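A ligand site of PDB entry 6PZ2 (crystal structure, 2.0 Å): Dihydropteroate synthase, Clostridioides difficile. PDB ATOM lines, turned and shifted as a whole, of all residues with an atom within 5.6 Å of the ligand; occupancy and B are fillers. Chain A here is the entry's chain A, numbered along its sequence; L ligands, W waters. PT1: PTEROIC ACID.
Water W1 bridges an oxygen (O22) of the ligand (2.6 Å) and the backbone carbonyl oxygen of Gly 181 (2.9 Å). Water W2 lies within hydrogen-bond range of O22 of the ligand (2.8 Å), N of Val 215 (3.0 Å) and OG of Ser 214 (3.1 Å).
OD2 of Asp 177 lies within hydrogen-bond range of N4 of the ligand (2.6 Å). The side-chain amino group (NZ) of Lys 213 sits at hydrogen-bond distance from an oxygen (O1) of the ligand, at 2.7 Å. N of Ser 214 sits at hydrogen-bond distance from O23 of the ligand (2.9 Å). The side-chain hydroxyl (OG) of Ser 214 is in hydrogen-bond range of an oxygen (O22) of the ligand (2.8 Å). N11 of the ligand lies within hydrogen-bond range of OD1 of Asn 112, at 2.8 Å. O1 of the ligand sits at hydrogen-bond distance from O of Gly 209 (3.2 Å). The guanidinium group (NE) of Arg 247 sits close to a nitrogen (N8) of the ligand (3.5 Å). The side-chain sulfur of Cys 135 is in hydrogen-bond range of a nitrogen (N11) of the ligand (3.7 Å).
N8 of the ligand sits close to OD2 of Asp 93, 3.1 Å away. The side-chain sulfur (SD) of Met 137 sits close to a nitrogen (N4) of the ligand (3.5 Å). Residues that only touch the ligand: Thr 59 (3.1 Å), Arg 60 (3.96 Å), Pro 61 (3.5 Å), Val 114 (3.7 Å), Gly 181 (3.6 Å), Phe 182 (3.3 Å) and Leu 207 (3.6 Å). Hydrophobic or aromatic side chains within 4 Å of the ligand: Pro 61, Val 114, Met 137, Phe 182 and Leu 207.
The side-chain carboxylate of Asp 177 sits at hydrogen-bond distance from the backbone NH of Gly 179. The backbone carbonyl oxygen of Gly 209 is in hydrogen-bond range of the side-chain amino group of Lys 213, 2.8 Å away. The side-chain amino group (NZ) of Lys 213 sits at hydrogen-bond distance from the backbone carbonyl oxygen (O) of Val 180 (2.7 Å). O of Lys 213 sits at hydrogen-bond distance from NH1 of Arg 227. The side-chain sulfur of Cys 135 sits close to the side-chain amide oxygen of Asn 112 (3.7 Å). ND2 of Asn 112 is in hydrogen-bond range of OD2 of Asp 53 (3.0 Å). The guanidinium group (NE) of Arg 247 lies within salt-bridge range of the side-chain carboxylate (OD2) of Asp 53. The backbone NH (N) of Arg 247 lies within hydrogen-bond range of the backbone carbonyl oxygen (O) of Leu 208 (2.9 Å).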
ATOM      1  N   ASP A  53     -29.522  -3.622  -3.484  1.00  0.00           N
ATOM      2  CA  ASP A  53     -29.634  -4.298  -4.738  1.00  0.00           C
ATOM      3  C   ASP A  53     -28.367  -5.141  -4.894  1.00  0.00           C
ATOM      4  O   ASP A  53     -27.298  -4.609  -5.225  1.00  0.00           O
ATOM      5  CB  ASP A  53     -29.753  -3.352  -5.938  1.00  0.00           C
ATOM      6  CG  ASP A  53     -30.120  -3.987  -7.266  1.00  0.00           C
ATOM      7  OD1 ASP A  53     -31.078  -4.802  -7.288  1.00  0.00           O
ATOM      8  OD2 ASP A  53     -29.483  -3.634  -8.294  1.00  0.00           O
ATOM      9  N   THR A  59     -24.084  -6.259 -14.965  1.00  0.00           N
ATOM     10  CA  THR A  59     -24.688  -5.811 -16.247  1.00  0.00           C
ATOM     11  C   THR A  59     -24.020  -4.529 -16.780  1.00  0.00           C
ATOM     12  O   THR A  59     -24.429  -3.977 -17.781  1.00  0.00           O
ATOM     13  CB  THR A  59     -26.196  -5.616 -16.064  1.00  0.00           C
ATOM     14  OG1 THR A  59     -26.351  -4.467 -15.239  1.00  0.00           O
ATOM     15  CG2 THR A  59     -26.871  -6.784 -15.367  1.00  0.00           C
ATOM     16  N   ARG A  60     -22.988  -4.069 -16.091  1.00  0.00           N
ATOM     17  CA  ARG A  60     -22.103  -3.042 -16.581  1.00  0.00           C
ATOM     18  C   ARG A  60     -21.466  -3.500 -17.900  1.00  0.00           C
ATOM     19  O   ARG A  60     -21.038  -4.629 -18.009  1.00  0.00           O
ATOM     20  CB  ARG A  60     -21.046  -2.802 -15.505  1.00  0.00           C
ATOM     21  CG  ARG A  60     -20.268  -1.518 -15.681  1.00  0.00           C
ATOM     22  CD  ARG A  60     -19.238  -1.436 -14.588  1.00  0.00           C
ATOM     23  NE  ARG A  60     -19.761  -1.254 -13.240  1.00  0.00           N
ATOM     24  CZ  ARG A  60     -18.959  -1.261 -12.183  1.00  0.00           C
ATOM     25  NH1 ARG A  60     -17.691  -1.585 -12.317  1.00  0.00           N
ATOM     26  NH2 ARG A  60     -19.403  -0.921 -10.999  1.00  0.00           N
ATOM     27  N   PRO A  61     -21.395  -2.627 -18.911  1.00  0.00           N
ATOM     28  CA  PRO A  61     -20.991  -3.026 -20.273  1.00  0.00           C
ATOM     29  C   PRO A  61     -19.652  -3.784 -20.415  1.00  0.00           C
ATOM     30  O   PRO A  61     -18.676  -3.447 -19.767  1.00  0.00           O
ATOM     31  CB  PRO A  61     -20.894  -1.691 -21.026  1.00  0.00           C
ATOM     32  CG  PRO A  61     -21.886  -0.794 -20.324  1.00  0.00           C
ATOM     33  CD  PRO A  61     -21.833  -1.227 -18.869  1.00  0.00           C
ATOM     34  N   ASP A  93     -30.624  -8.403  -8.255  1.00  0.00           N
ATOM     35  CA  ASP A  93     -30.386  -7.878  -9.560  1.00  0.00           C
ATOM     36  C   ASP A  93     -30.082  -9.091 -10.442  1.00  0.00           C
ATOM     37  O   ASP A  93     -28.939  -9.478 -10.554  1.00  0.00           O
ATOM     38  CB  ASP A  93     -29.200  -6.906  -9.555  1.00  0.00           C
ATOM     39  CG  ASP A  93     -28.939  -6.178 -10.869  1.00  0.00           C
ATOM     40  OD1 ASP A  93     -29.117  -6.765 -11.973  1.00  0.00           O
ATOM     41  OD2 ASP A  93     -28.525  -5.012 -10.761  1.00  0.00           O
ATOM     42  N   ASN A 112     -35.022  -7.253  -9.451  1.00  0.00           N
ATOM     43  CA  ASN A 112     -34.619  -6.205 -10.302  1.00  0.00           C
ATOM     44  C   ASN A 112     -34.174  -6.815 -11.644  1.00  0.00           C
ATOM     45  O   ASN A 112     -33.014  -7.200 -11.783  1.00  0.00           O
ATOM     46  CB  ASN A 112     -33.499  -5.405  -9.635  1.00  0.00           C
ATOM     47  CG  ASN A 112     -33.004  -4.262 -10.500  1.00  0.00           C
ATOM     48  OD1 ASN A 112     -33.749  -3.808 -11.358  1.00  0.00           O
ATOM     49  ND2 ASN A 112     -31.769  -3.810 -10.281  1.00  0.00           N
ATOM     50  N   VAL A 114     -33.058  -6.455 -15.358  1.00  0.00           N
ATOM     51  CA  VAL A 114     -32.547  -5.510 -16.357  1.00  0.00           C
ATOM     52  C   VAL A 114     -32.912  -5.933 -17.777  1.00  0.00           C
ATOM     53  O   VAL A 114     -32.443  -5.273 -18.709  1.00  0.00           O
ATOM     54  CB  VAL A 114     -31.024  -5.289 -16.263  1.00  0.00           C
ATOM     55  CG1 VAL A 114     -30.610  -4.750 -14.895  1.00  0.00           C
ATOM     56  CG2 VAL A 114     -30.245  -6.546 -16.618  1.00  0.00           C
ATOM     57  N   CYS A 135     -38.899  -4.785 -10.490  1.00  0.00           N
ATOM     58  CA  CYS A 135     -38.524  -3.681 -11.290  1.00  0.00           C
ATOM     59  C   CYS A 135     -38.352  -4.172 -12.724  1.00  0.00           C
ATOM     60  O   CYS A 135     -37.457  -4.942 -13.024  1.00  0.00           O
ATOM     61  CB  CYS A 135     -37.243  -3.014 -10.793  1.00  0.00           C
ATOM     62  SG  CYS A 135     -36.719  -1.612 -11.816  1.00  0.00           S
ATOM     63  N   MET A 137     -37.178  -3.085 -16.177  1.00  0.00           N
ATOM     64  CA  MET A 137     -36.325  -2.121 -16.760  1.00  0.00           C
ATOM     65  C   MET A 137     -36.334  -2.279 -18.286  1.00  0.00           C
ATOM     66  O   MET A 137     -36.307  -3.383 -18.773  1.00  0.00           O
ATOM     67  CB  MET A 137     -34.885  -2.295 -16.253  1.00  0.00           C
ATOM     68  CG  MET A 137     -34.011  -1.109 -16.573  1.00  0.00           C
ATOM     69  SD  MET A 137     -32.245  -1.376 -16.359  1.00  0.00           S
ATOM     70  CE  MET A 137     -31.834  -2.097 -17.955  1.00  0.00           C
ATOM     71  N   ASP A 177     -38.430   1.307 -14.923  1.00  0.00           N
ATOM     72  CA  ASP A 177     -37.162   1.941 -14.981  1.00  0.00           C
ATOM     73  C   ASP A 177     -36.772   2.062 -16.457  1.00  0.00           C
ATOM     74  O   ASP A 177     -36.825   1.066 -17.165  1.00  0.00           O
ATOM     75  CB  ASP A 177     -36.118   1.118 -14.227  1.00  0.00           C
ATOM     76  CG  ASP A 177     -34.692   1.649 -14.278  1.00  0.00           C
ATOM     77  OD1 ASP A 177     -34.377   2.433 -15.196  1.00  0.00           O
ATOM     78  OD2 ASP A 177     -33.891   1.244 -13.392  1.00  0.00           O
ATOM     79  N   GLY A 179     -33.957   2.538 -17.939  1.00  0.00           N
ATOM     80  CA  GLY A 179     -32.768   1.796 -18.383  1.00  0.00           C
ATOM     81  C   GLY A 179     -31.736   2.708 -19.010  1.00  0.00           C
ATOM     82  O   GLY A 179     -31.248   2.478 -20.120  1.00  0.00           O
ATOM     83  N   VAL A 180     -31.318   3.701 -18.239  1.00  0.00           N
ATOM     84  CA  VAL A 180     -30.257   4.599 -18.719  1.00  0.00           C
ATOM     85  C   VAL A 180     -29.003   3.772 -18.967  1.00  0.00           C
ATOM     86  O   VAL A 180     -28.562   3.034 -18.121  1.00  0.00           O
ATOM     87  CB  VAL A 180     -29.982   5.773 -17.746  1.00  0.00           C
ATOM     88  CG1 VAL A 180     -28.778   6.602 -18.157  1.00  0.00           C
ATOM     89  CG2 VAL A 180     -31.197   6.673 -17.591  1.00  0.00           C
ATOM     90  N   GLY A 181     -28.392   3.939 -20.132  1.00  0.00           N
ATOM     91  CA  GLY A 181     -27.165   3.234 -20.404  1.00  0.00           C
ATOM     92  C   GLY A 181     -27.383   1.890 -21.104  1.00  0.00           C
ATOM     93  O   GLY A 181     -26.393   1.223 -21.440  1.00  0.00           O
ATOM     94  N   PHE A 182     -28.627   1.511 -21.358  1.00  0.00           N
ATOM     95  CA  PHE A 182     -28.907   0.200 -21.937  1.00  0.00           C
ATOM     96  C   PHE A 182     -29.640   0.379 -23.259  1.00  0.00           C
ATOM     97  O   PHE A 182     -30.758   0.921 -23.303  1.00  0.00           O
ATOM     98  CB  PHE A 182     -29.813  -0.628 -21.024  1.00  0.00           C
ATOM     99  CG  PHE A 182     -29.235  -1.074 -19.698  1.00  0.00           C
ATOM    100  CD1 PHE A 182     -29.430  -0.321 -18.555  1.00  0.00           C
ATOM    101  CD2 PHE A 182     -28.609  -2.306 -19.583  1.00  0.00           C
ATOM    102  CE1 PHE A 182     -28.950  -0.767 -17.326  1.00  0.00           C
ATOM    103  CE2 PHE A 182     -28.117  -2.735 -18.365  1.00  0.00           C
ATOM    104  CZ  PHE A 182     -28.305  -1.976 -17.231  1.00  0.00           C
ATOM    105  N   LEU A 207     -38.041   3.902 -11.043  1.00  0.00           N
ATOM    106  CA  LEU A 207     -36.728   3.728 -10.522  1.00  0.00           C
ATOM    107  C   LEU A 207     -35.719   4.204 -11.563  1.00  0.00           C
ATOM    108  O   LEU A 207     -35.884   3.909 -12.763  1.00  0.00           O
ATOM    109  CB  LEU A 207     -36.494   2.269 -10.143  1.00  0.00           C
ATOM    110  CG  LEU A 207     -35.195   1.943  -9.403  1.00  0.00           C
ATOM    111  CD1 LEU A 207     -35.367   0.707  -8.542  1.00  0.00           C
ATOM    112  CD2 LEU A 207     -34.064   1.712 -10.375  1.00  0.00           C
ATOM    113  N   LEU A 208     -34.709   4.912 -11.091  1.00  0.00           N
ATOM    114  CA  LEU A 208     -33.695   5.474 -12.003  1.00  0.00           C
ATOM    115  C   LEU A 208     -32.295   5.053 -11.555  1.00  0.00           C
ATOM    116  O   LEU A 208     -31.956   5.123 -10.366  1.00  0.00           O
ATOM    117  CB  LEU A 208     -33.834   7.001 -12.049  1.00  0.00           C
ATOM    118  CG  LEU A 208     -32.792   7.707 -12.904  1.00  0.00           C
ATOM    119  CD1 LEU A 208     -33.002   7.336 -14.362  1.00  0.00           C
ATOM    120  CD2 LEU A 208     -32.858   9.223 -12.735  1.00  0.00           C
ATOM    121  N   GLY A 209     -31.479   4.670 -12.522  1.00  0.00           N
ATOM    122  CA  GLY A 209     -30.087   4.437 -12.222  1.00  0.00           C
ATOM    123  C   GLY A 209     -29.148   5.064 -13.238  1.00  0.00           C
ATOM    124  O   GLY A 209     -29.209   4.717 -14.415  1.00  0.00           O
ATOM    125  N   THR A 210     -28.283   5.957 -12.763  1.00  0.00           N
ATOM    126  CA  THR A 210     -27.315   6.699 -13.597  1.00  0.00           C
ATOM    127  C   THR A 210     -25.916   6.655 -12.985  1.00  0.00           C
ATOM    128  O   THR A 210     -24.940   6.958 -13.661  1.00  0.00           O
ATOM    129  CB  THR A 210     -27.682   8.181 -13.761  1.00  0.00           C
ATOM    130  OG1 THR A 210     -27.593   8.806 -12.470  1.00  0.00           O
ATOM    131  CG2 THR A 210     -29.069   8.363 -14.334  1.00  0.00           C
ATOM    132  N   ARG A 212     -22.516   6.817 -11.864  1.00  0.00           N
ATOM    133  CA  ARG A 212     -21.169   6.593 -12.413  1.00  0.00           C
ATOM    134  C   ARG A 212     -21.202   6.185 -13.885  1.00  0.00           C
ATOM    135  O   ARG A 212     -20.154   5.880 -14.405  1.00  0.00           O
ATOM    136  CB  ARG A 212     -20.390   5.541 -11.630  1.00  0.00           C
ATOM    137  CG  ARG A 212     -20.147   5.953 -10.190  1.00  0.00           C
ATOM    138  CD  ARG A 212     -19.284   4.954  -9.447  1.00  0.00           C
ATOM    139  NE  ARG A 212     -19.329   5.379  -8.056  1.00  0.00           N
ATOM    140  CZ  ARG A 212     -18.773   4.692  -7.081  1.00  0.00           C
ATOM    141  NH1 ARG A 212     -18.143   3.581  -7.403  1.00  0.00           N
ATOM    142  NH2 ARG A 212     -18.837   5.120  -5.817  1.00  0.00           N
ATOM    143  N   LYS A 213     -22.335   6.244 -14.559  1.00  0.00           N
ATOM    144  CA  LYS A 213     -22.401   5.711 -15.910  1.00  0.00           C
ATOM    145  C   LYS A 213     -21.686   6.634 -16.901  1.00  0.00           C
ATOM    146  O   LYS A 213     -21.388   7.792 -16.620  1.00  0.00           O
ATOM    147  CB  LYS A 213     -23.858   5.489 -16.318  1.00  0.00           C
ATOM    148  CG  LYS A 213     -24.522   4.394 -15.508  1.00  0.00           C
ATOM    149  CD  LYS A 213     -25.837   3.912 -16.049  1.00  0.00           C
ATOM    150  CE  LYS A 213     -26.501   2.983 -15.065  1.00  0.00           C
ATOM    151  NZ  LYS A 213     -27.832   2.565 -15.551  1.00  0.00           N
ATOM    152  N   SER A 214     -21.426   6.069 -18.073  1.00  0.00           N
ATOM    153  CA  SER A 214     -20.671   6.719 -19.132  1.00  0.00           C
ATOM    154  C   SER A 214     -21.448   7.921 -19.688  1.00  0.00           C
ATOM    155  O   SER A 214     -20.867   8.814 -20.266  1.00  0.00           O
ATOM    156  CB  SER A 214     -20.376   5.749 -20.235  1.00  0.00           C
ATOM    157  OG  SER A 214     -21.593   5.464 -20.917  1.00  0.00           O
ATOM    158  N   VAL A 215     -22.764   7.944 -19.544  1.00  0.00           N
ATOM    159  CA  VAL A 215     -23.510   9.141 -19.955  1.00  0.00           C
ATOM    160  C   VAL A 215     -23.079  10.377 -19.139  1.00  0.00           C
ATOM    161  O   VAL A 215     -23.046  11.493 -19.656  1.00  0.00           O
ATOM    162  CB  VAL A 215     -25.037   8.974 -19.858  1.00  0.00           C
ATOM    163  CG1 VAL A 215     -25.511   8.696 -18.429  1.00  0.00           C
ATOM    164  CG2 VAL A 215     -25.752  10.199 -20.410  1.00  0.00           C
ATOM    165  N   ARG A 227     -17.583  11.007 -10.621  1.00  0.00           N
ATOM    166  CA  ARG A 227     -18.744  11.558 -11.316  1.00  0.00           C
ATOM    167  C   ARG A 227     -19.895  11.848 -10.347  1.00  0.00           C
ATOM    168  O   ARG A 227     -21.000  12.102 -10.782  1.00  0.00           O
ATOM    169  CB  ARG A 227     -19.186  10.591 -12.420  1.00  0.00           C
ATOM    170  CG  ARG A 227     -18.072  10.300 -13.408  1.00  0.00           C
ATOM    171  CD  ARG A 227     -18.402   9.167 -14.350  1.00  0.00           C
ATOM    172  NE  ARG A 227     -17.226   8.968 -15.181  1.00  0.00           N
ATOM    173  CZ  ARG A 227     -17.065   7.982 -16.046  1.00  0.00           C
ATOM    174  NH1 ARG A 227     -18.035   7.127 -16.284  1.00  0.00           N
ATOM    175  NH2 ARG A 227     -15.910   7.874 -16.680  1.00  0.00           N
ATOM    176  N   ARG A 247     -31.141   4.274  -7.742  1.00  0.00           N
ATOM    177  CA  ARG A 247     -30.171   3.222  -7.485  1.00  0.00           C
ATOM    178  C   ARG A 247     -28.785   3.856  -7.585  1.00  0.00           C
ATOM    179  O   ARG A 247     -28.390   4.215  -8.683  1.00  0.00           O
ATOM    180  CB  ARG A 247     -30.326   2.115  -8.552  1.00  0.00           C
ATOM    181  CG  ARG A 247     -29.369   0.933  -8.453  1.00  0.00           C
ATOM    182  CD  ARG A 247     -29.579  -0.116  -9.541  1.00  0.00           C
ATOM    183  NE  ARG A 247     -28.644  -1.237  -9.539  1.00  0.00           N
ATOM    184  CZ  ARG A 247     -27.409  -1.206 -10.007  1.00  0.00           C
ATOM    185  NH1 ARG A 247     -26.926  -0.126 -10.617  1.00  0.00           N
ATOM    186  NH2 ARG A 247     -26.634  -2.270  -9.849  1.00  0.00           N
HETATM  187  C2  PT1 L   1     -30.267   0.475 -13.723  1.00  0.00           C
HETATM  188  C3  PT1 L   1     -29.170  -0.460 -13.571  1.00  0.00           C
HETATM  189  C5  PT1 L   1     -29.529  -1.697 -12.877  1.00  0.00           C
HETATM  190  N6  PT1 L   1     -27.894  -0.258 -13.994  1.00  0.00           N
HETATM  191  C7  PT1 L   1     -31.759  -0.985 -12.676  1.00  0.00           C
HETATM  192  N9  PT1 L   1     -30.792  -1.897 -12.495  1.00  0.00           N
HETATM  193  C10 PT1 L   1     -26.964  -1.210 -13.809  1.00  0.00           C
HETATM  194  N11 PT1 L   1     -33.016  -1.213 -12.237  1.00  0.00           N
HETATM  195  C12 PT1 L   1     -27.308  -2.416 -13.186  1.00  0.00           C
HETATM  196  C21 PT1 L   1     -22.436   2.789 -18.718  1.00  0.00           C
HETATM  197  O22 PT1 L   1     -22.891   3.277 -19.770  1.00  0.00           O
HETATM  198  O1  PT1 L   1     -30.092   1.653 -14.333  1.00  0.00           O
HETATM  199  N4  PT1 L   1     -31.516   0.179 -13.306  1.00  0.00           N
HETATM  200  N8  PT1 L   1     -28.561  -2.620 -12.703  1.00  0.00           N
HETATM  201  C13 PT1 L   1     -25.555  -0.975 -14.322  1.00  0.00           C
HETATM  202  N14 PT1 L   1     -25.623  -0.799 -15.762  1.00  0.00           N
HETATM  203  C15 PT1 L   1     -24.802   0.027 -16.452  1.00  0.00           C
HETATM  204  C16 PT1 L   1     -23.634   0.558 -15.884  1.00  0.00           C
HETATM  205  C17 PT1 L   1     -25.176   0.402 -17.733  1.00  0.00           C
HETATM  206  C18 PT1 L   1     -22.854   1.432 -16.643  1.00  0.00           C
HETATM  207  C19 PT1 L   1     -24.396   1.276 -18.492  1.00  0.00           C
HETATM  208  C20 PT1 L   1     -23.234   1.797 -17.936  1.00  0.00           C
HETATM  209  O23 PT1 L   1     -21.348   3.183 -18.294  1.00  0.00           O
HETATM  210  O   HOH W   1     -23.837   2.358 -22.054  1.00  0.00           O
HETATM  211  O   HOH W   2     -24.538   5.520 -19.890  1.00  0.00           O
HETATM  212  O   HOH W   3     -31.918   3.615 -15.363  1.00  0.00           O
